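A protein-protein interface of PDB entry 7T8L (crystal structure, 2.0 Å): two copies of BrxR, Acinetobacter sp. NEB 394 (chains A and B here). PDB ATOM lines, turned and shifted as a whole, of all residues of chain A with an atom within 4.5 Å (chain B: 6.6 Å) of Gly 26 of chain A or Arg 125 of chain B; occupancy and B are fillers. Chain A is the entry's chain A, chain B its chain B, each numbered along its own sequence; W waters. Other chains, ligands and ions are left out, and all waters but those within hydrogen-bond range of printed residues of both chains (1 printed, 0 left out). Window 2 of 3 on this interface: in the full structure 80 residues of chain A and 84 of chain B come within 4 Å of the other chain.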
ATOM      1  N   LEU A  21       8.808 -18.759   6.435  1.00  0.00           N
ATOM      2  CA  LEU A  21       9.239 -19.825   5.487  1.00  0.00           C
ATOM      3  C   LEU A  21      10.170 -19.226   4.436  1.00  0.00           C
ATOM      4  O   LEU A  21      11.245 -19.845   4.187  1.00  0.00           O
ATOM      5  CB  LEU A  21       8.039 -20.505   4.825  1.00  0.00           C
ATOM      6  CG  LEU A  21       7.302 -21.503   5.702  1.00  0.00           C
ATOM      7  CD1 LEU A  21       5.998 -21.916   5.050  1.00  0.00           C
ATOM      8  CD2 LEU A  21       8.192 -22.704   6.008  1.00  0.00           C
ATOM      9  N   ALA A  22       9.793 -18.092   3.832  1.00  0.00           N
ATOM     10  CA  ALA A  22      10.624 -17.395   2.820  1.00  0.00           C
ATOM     11  C   ALA A  22      11.996 -17.059   3.416  1.00  0.00           C
ATOM     12  O   ALA A  22      13.053 -17.288   2.760  1.00  0.00           O
ATOM     13  CB  ALA A  22       9.955 -16.132   2.301  1.00  0.00           C
ATOM     14  N   TYR A  23      11.993 -16.455   4.583  1.00  0.00           N
ATOM     15  CA  TYR A  23      13.217 -15.862   5.160  1.00  0.00           C
ATOM     16  C   TYR A  23      14.164 -16.941   5.690  1.00  0.00           C
ATOM     17  O   TYR A  23      15.395 -16.831   5.427  1.00  0.00           O
ATOM     18  CB  TYR A  23      12.834 -14.903   6.265  1.00  0.00           C
ATOM     19  CG  TYR A  23      13.972 -14.041   6.727  1.00  0.00           C
ATOM     20  CD1 TYR A  23      14.649 -13.215   5.845  1.00  0.00           C
ATOM     21  CD2 TYR A  23      14.396 -14.081   8.038  1.00  0.00           C
ATOM     22  CE1 TYR A  23      15.690 -12.408   6.277  1.00  0.00           C
ATOM     23  CE2 TYR A  23      15.418 -13.268   8.487  1.00  0.00           C
ATOM     24  CZ  TYR A  23      16.076 -12.438   7.602  1.00  0.00           C
ATOM     25  OH  TYR A  23      17.098 -11.664   8.066  1.00  0.00           O
ATOM     26  N   TRP A  24      13.629 -17.920   6.420  1.00  0.00           N
ATOM     27  CA  TRP A  24      14.430 -18.950   7.139  1.00  0.00           C
ATOM     28  C   TRP A  24      14.713 -20.158   6.236  1.00  0.00           C
ATOM     29  O   TRP A  24      15.817 -20.727   6.340  1.00  0.00           O
ATOM     30  CB  TRP A  24      13.784 -19.300   8.498  1.00  0.00           C
ATOM     31  CG  TRP A  24      13.908 -18.146   9.442  1.00  0.00           C
ATOM     32  CD1 TRP A  24      12.927 -17.259   9.788  1.00  0.00           C
ATOM     33  CD2 TRP A  24      15.108 -17.673  10.081  1.00  0.00           C
ATOM     34  NE1 TRP A  24      13.426 -16.293  10.624  1.00  0.00           N
ATOM     35  CE2 TRP A  24      14.760 -16.526  10.828  1.00  0.00           C
ATOM     36  CE3 TRP A  24      16.428 -18.138  10.153  1.00  0.00           C
ATOM     37  CZ2 TRP A  24      15.692 -15.816  11.578  1.00  0.00           C
ATOM     38  CZ3 TRP A  24      17.349 -17.439  10.905  1.00  0.00           C
ATOM     39  CH2 TRP A  24      16.986 -16.293  11.605  1.00  0.00           C
ATOM     40  N   GLU A  25      13.769 -20.588   5.407  1.00  0.00           N
ATOM     41  CA  GLU A  25      13.925 -21.786   4.518  1.00  0.00           C
ATOM     42  C   GLU A  25      14.325 -21.359   3.097  1.00  0.00           C
ATOM     43  O   GLU A  25      14.929 -22.172   2.404  1.00  0.00           O
ATOM     44  CB  GLU A  25      12.673 -22.648   4.565  1.00  0.00           C
ATOM     45  CG  GLU A  25      12.298 -23.074   5.971  1.00  0.00           C
ATOM     46  CD  GLU A  25      11.344 -24.255   6.071  1.00  0.00           C
ATOM     47  OE1 GLU A  25      10.996 -24.835   5.023  1.00  0.00           O
ATOM     48  OE2 GLU A  25      10.951 -24.624   7.203  1.00  0.00           O
ATOM     49  N   GLY A  26      14.059 -20.112   2.690  1.00  0.00           N
ATOM     50  CA  GLY A  26      14.432 -19.578   1.362  1.00  0.00           C
ATOM     51  C   GLY A  26      13.483 -20.029   0.262  1.00  0.00           C
ATOM     52  O   GLY A  26      13.794 -19.843  -0.918  1.00  0.00           O
ATOM     53  N   ARG A  27      12.357 -20.624   0.629  1.00  0.00           N
ATOM     54  CA  ARG A  27      11.401 -21.250  -0.311  1.00  0.00           C
ATOM     55  C   ARG A  27      10.038 -21.375   0.373  1.00  0.00           C
ATOM     56  O   ARG A  27       9.995 -21.720   1.536  1.00  0.00           O
ATOM     57  CB  ARG A  27      11.900 -22.622  -0.768  1.00  0.00           C
ATOM     58  CG  ARG A  27      10.964 -23.277  -1.773  1.00  0.00           C
ATOM     59  CD  ARG A  27      11.423 -24.630  -2.285  1.00  0.00           C
ATOM     60  NE  ARG A  27      12.816 -24.593  -2.708  1.00  0.00           N
ATOM     61  CZ  ARG A  27      13.571 -25.665  -2.937  1.00  0.00           C
ATOM     62  NH1 ARG A  27      13.066 -26.882  -2.782  1.00  0.00           N
ATOM     63  NH2 ARG A  27      14.831 -25.511  -3.313  1.00  0.00           N
ATOM     64  N   VAL A  70      10.128 -17.928  -4.092  1.00  0.00           N
ATOM     65  CA  VAL A  70      11.481 -17.674  -3.534  1.00  0.00           C
ATOM     66  C   VAL A  70      11.554 -16.191  -3.204  1.00  0.00           C
ATOM     67  O   VAL A  70      10.954 -15.386  -3.905  1.00  0.00           O
ATOM     68  CB  VAL A  70      12.553 -18.135  -4.549  1.00  0.00           C
ATOM     69  CG1 VAL A  70      12.270 -17.606  -5.945  1.00  0.00           C
ATOM     70  CG2 VAL A  70      13.965 -17.773  -4.135  1.00  0.00           C
ATOM     71  N   PRO A  71      12.257 -15.769  -2.130  1.00  0.00           N
ATOM     72  CA  PRO A  71      12.470 -14.345  -1.879  1.00  0.00           C
ATOM     73  C   PRO A  71      13.339 -13.681  -2.960  1.00  0.00           C
ATOM     74  O   PRO A  71      14.344 -14.271  -3.315  1.00  0.00           O
ATOM     75  CB  PRO A  71      13.211 -14.304  -0.535  1.00  0.00           C
ATOM     76  CG  PRO A  71      13.853 -15.671  -0.422  1.00  0.00           C
ATOM     77  CD  PRO A  71      12.872 -16.616  -1.093  1.00  0.00           C
ATOM     78  N   ARG B 120      22.316 -16.948  11.563  1.00  0.00           N
ATOM     79  CA  ARG B 120      21.995 -16.276  10.283  1.00  0.00           C
ATOM     80  C   ARG B 120      21.032 -17.110   9.438  1.00  0.00           C
ATOM     81  O   ARG B 120      21.192 -18.328   9.216  1.00  0.00           O
ATOM     82  CB  ARG B 120      23.312 -15.858   9.613  1.00  0.00           C
ATOM     83  CG  ARG B 120      24.050 -14.765  10.381  1.00  0.00           C
ATOM     84  CD  ARG B 120      25.333 -14.258   9.716  1.00  0.00           C
ATOM     85  NE  ARG B 120      26.293 -15.353   9.623  1.00  0.00           N
ATOM     86  CZ  ARG B 120      26.605 -16.060   8.526  1.00  0.00           C
ATOM     87  NH1 ARG B 120      26.068 -15.782   7.347  1.00  0.00           N
ATOM     88  NH2 ARG B 120      27.464 -17.064   8.628  1.00  0.00           N
ATOM     89  N   PRO B 121      20.041 -16.414   8.822  1.00  0.00           N
ATOM     90  CA  PRO B 121      19.126 -17.024   7.867  1.00  0.00           C
ATOM     91  C   PRO B 121      19.800 -17.786   6.713  1.00  0.00           C
ATOM     92  O   PRO B 121      19.319 -18.840   6.344  1.00  0.00           O
ATOM     93  CB  PRO B 121      18.304 -15.864   7.276  1.00  0.00           C
ATOM     94  CG  PRO B 121      18.697 -14.614   8.020  1.00  0.00           C
ATOM     95  CD  PRO B 121      19.813 -14.964   8.978  1.00  0.00           C
ATOM     96  N   GLU B 122      20.909 -17.265   6.185  1.00  0.00           N
ATOM     97  CA  GLU B 122      21.600 -17.867   5.015  1.00  0.00           C
ATOM     98  C   GLU B 122      22.191 -19.212   5.440  1.00  0.00           C
ATOM     99  O   GLU B 122      22.280 -20.117   4.598  1.00  0.00           O
ATOM    100  CB  GLU B 122      22.635 -16.906   4.408  1.00  0.00           C
ATOM    101  CG  GLU B 122      23.526 -16.194   5.423  1.00  0.00           C
ATOM    102  CD  GLU B 122      23.046 -14.842   5.962  1.00  0.00           C
ATOM    103  OE1 GLU B 122      21.840 -14.699   6.309  1.00  0.00           O
ATOM    104  OE2 GLU B 122      23.893 -13.924   6.060  1.00  0.00           O
ATOM    105  N   VAL B 123      22.577 -19.350   6.705  1.00  0.00           N
ATOM    106  CA  VAL B 123      23.118 -20.620   7.261  1.00  0.00           C
ATOM    107  C   VAL B 123      21.965 -21.615   7.442  1.00  0.00           C
ATOM    108  O   VAL B 123      22.073 -22.763   6.955  1.00  0.00           O
ATOM    109  CB  VAL B 123      23.896 -20.364   8.565  1.00  0.00           C
ATOM    110  CG1 VAL B 123      24.325 -21.661   9.230  1.00  0.00           C
ATOM    111  CG2 VAL B 123      25.095 -19.481   8.300  1.00  0.00           C
ATOM    112  N   ILE B 124      20.867 -21.203   8.080  1.00  0.00           N
ATOM    113  CA  ILE B 124      19.702 -22.098   8.319  1.00  0.00           C
ATOM    114  C   ILE B 124      19.210 -22.619   6.979  1.00  0.00           C
ATOM    115  O   ILE B 124      18.912 -23.845   6.877  1.00  0.00           O
ATOM    116  CB  ILE B 124      18.584 -21.372   9.088  1.00  0.00           C
ATOM    117  CG1 ILE B 124      18.994 -21.060  10.516  1.00  0.00           C
ATOM    118  CG2 ILE B 124      17.308 -22.197   9.046  1.00  0.00           C
ATOM    119  CD1 ILE B 124      19.377 -22.259  11.321  1.00  0.00           C
ATOM    120  N   ARG B 125      19.031 -21.713   6.015  1.00  0.00           N
ATOM    121  CA  ARG B 125      18.483 -22.083   4.685  1.00  0.00           C
ATOM    122  C   ARG B 125      19.293 -23.266   4.147  1.00  0.00           C
ATOM    123  O   ARG B 125      18.679 -24.251   3.719  1.00  0.00           O
ATOM    124  CB  ARG B 125      18.576 -20.942   3.667  1.00  0.00           C
ATOM    125  CG  ARG B 125      17.570 -19.826   3.908  1.00  0.00           C
ATOM    126  CD  ARG B 125      17.648 -18.713   2.896  1.00  0.00           C
ATOM    127  NE  ARG B 125      17.222 -17.445   3.449  1.00  0.00           N
ATOM    128  CZ  ARG B 125      17.443 -16.251   2.897  1.00  0.00           C
ATOM    129  NH1 ARG B 125      18.038 -16.147   1.715  1.00  0.00           N
ATOM    130  NH2 ARG B 125      17.060 -15.153   3.528  1.00  0.00           N
ATOM    131  N   GLU B 126      20.616 -23.158   4.164  1.00  0.00           N
ATOM    132  CA  GLU B 126      21.487 -24.185   3.531  1.00  0.00           C
ATOM    133  C   GLU B 126      21.489 -25.456   4.375  1.00  0.00           C
ATOM    134  O   GLU B 126      21.493 -26.560   3.795  1.00  0.00           O
ATOM    135  CB  GLU B 126      22.903 -23.657   3.321  1.00  0.00           C
ATOM    136  CG  GLU B 126      22.978 -22.660   2.189  1.00  0.00           C
ATOM    137  CD  GLU B 126      22.505 -23.242   0.862  1.00  0.00           C
ATOM    138  OE1 GLU B 126      22.949 -24.353   0.509  1.00  0.00           O
ATOM    139  OE2 GLU B 126      21.662 -22.603   0.220  1.00  0.00           O
ATOM    140  N   VAL B 127      21.531 -25.313   5.697  1.00  0.00           N
ATOM    141  CA  VAL B 127      21.719 -26.481   6.599  1.00  0.00           C
ATOM    142  C   VAL B 127      20.447 -27.322   6.534  1.00  0.00           C
ATOM    143  O   VAL B 127      20.535 -28.556   6.397  1.00  0.00           O
ATOM    144  CB  VAL B 127      22.120 -26.030   8.016  1.00  0.00           C
ATOM    145  CG1 VAL B 127      22.059 -27.172   9.014  1.00  0.00           C
ATOM    146  CG2 VAL B 127      23.517 -25.420   8.005  1.00  0.00           C
ATOM    147  N   LEU B 128      19.292 -26.672   6.617  1.00  0.00           N
ATOM    148  CA  LEU B 128      17.982 -27.347   6.560  1.00  0.00           C
ATOM    149  C   LEU B 128      17.791 -28.038   5.200  1.00  0.00           C
ATOM    150  O   LEU B 128      17.297 -29.194   5.161  1.00  0.00           O
ATOM    151  CB  LEU B 128      16.906 -26.298   6.815  1.00  0.00           C
ATOM    152  CG  LEU B 128      15.484 -26.828   6.889  1.00  0.00           C
ATOM    153  CD1 LEU B 128      15.340 -27.834   8.037  1.00  0.00           C
ATOM    154  CD2 LEU B 128      14.520 -25.649   7.064  1.00  0.00           C
ATOM    155  N   ARG B 129      18.133 -27.368   4.108  1.00  0.00           N
ATOM    156  CA  ARG B 129      18.038 -28.014   2.767  1.00  0.00           C
ATOM    157  C   ARG B 129      18.916 -29.283   2.716  1.00  0.00           C
ATOM    158  O   ARG B 129      18.456 -30.347   2.204  1.00  0.00           O
ATOM    159  CB  ARG B 129      18.419 -27.027   1.670  1.00  0.00           C
ATOM    160  CG  ARG B 129      18.182 -27.569   0.268  1.00  0.00           C
ATOM    161  CD  ARG B 129      18.392 -26.472  -0.758  1.00  0.00           C
ATOM    162  NE  ARG B 129      19.808 -26.224  -0.904  1.00  0.00           N
ATOM    163  N   ALA B 130      20.126 -29.206   3.255  1.00  0.00           N
ATOM    164  CA  ALA B 130      21.078 -30.342   3.286  1.00  0.00           C
ATOM    165  C   ALA B 130      20.563 -31.458   4.209  1.00  0.00           C
ATOM    166  O   ALA B 130      20.674 -32.661   3.831  1.00  0.00           O
ATOM    167  CB  ALA B 130      22.429 -29.803   3.675  1.00  0.00           C
HETATM  168  O   HOH W   1      15.941 -24.519   3.407  1.00  0.00           O
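O of Leu 21 of chain A is in hydrogen-bond range of N of Gly 26 of chain A (3.2 Å). The guanidinium group of Arg 120 of chain B is in salt-bridge range of the side-chain carboxylate of Glu 122 of chain B (3.1 Å).
Among the printed residues, merely in contact across the chains: Tyr 23 of chain A with Pro 121 of chain B, Trp 24 of chain A with Arg 120 of chain B, Trp 24 of chain A with Pro 121 of chain B, Trp 24 of chain A with Ile 124 of chain B, Glu 25 of chain A with Arg 125 of chain B, Glu 25 of chain A with Leu 128 of chain B and Gly 26 of chain A with Arg 125 of chain B.
No position is printed for both chains. Of the 9 pairs that touch across the chains among the printed residues, none has its exchanged pair printed and touching as well.
Printed residues of chain B that touch a printed residue of chain A: Arg 120, Pro 121, Ile 124, Arg 125 and Leu 128. Along chain B the printed residues that touch a printed residue of chain A span positions 120 to 128. Among the printed residues, 9 pairs touch across the chains. Among the printed residues, no Asp or Glu carboxylate lies within 4 Å of a Lys or Arg side-chain nitrogen of the other chain.
Of chain B, only Arg 125 (3.7 Å) comes within 4 Å of Gly 26 of chain A. Printed residues of chain A within 4 Å of Arg 120 of chain B: Trp 24 (3.98 Å). Of the printed residues of chain A, Pro 121 of chain B touches Tyr 23 (3.4 Å) and Trp 24 (3.5 Å). Arg 125 of chain B touches four residues of chain A. Arg 129 of chain B touches none of the printed residues of chain A. The nearest residue of chain A that does not touch Arg 125 of chain B is Ala 22 of chain A (4.2 Å).
The backbone carbonyl oxygen (O) of Tyr 23 of chain A lies within hydrogen-bond range of the guanidinium group (NE) of Arg 125 of chain B (2.8 Å). The backbone carbonyl oxygen (O) of Trp 24 of chain A sits close to the backbone NH (N) of Arg 125 of chain B (3.4 Å).
Water W1 bridges O of Glu 25 of chain A and O of Arg 125 of chain B.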
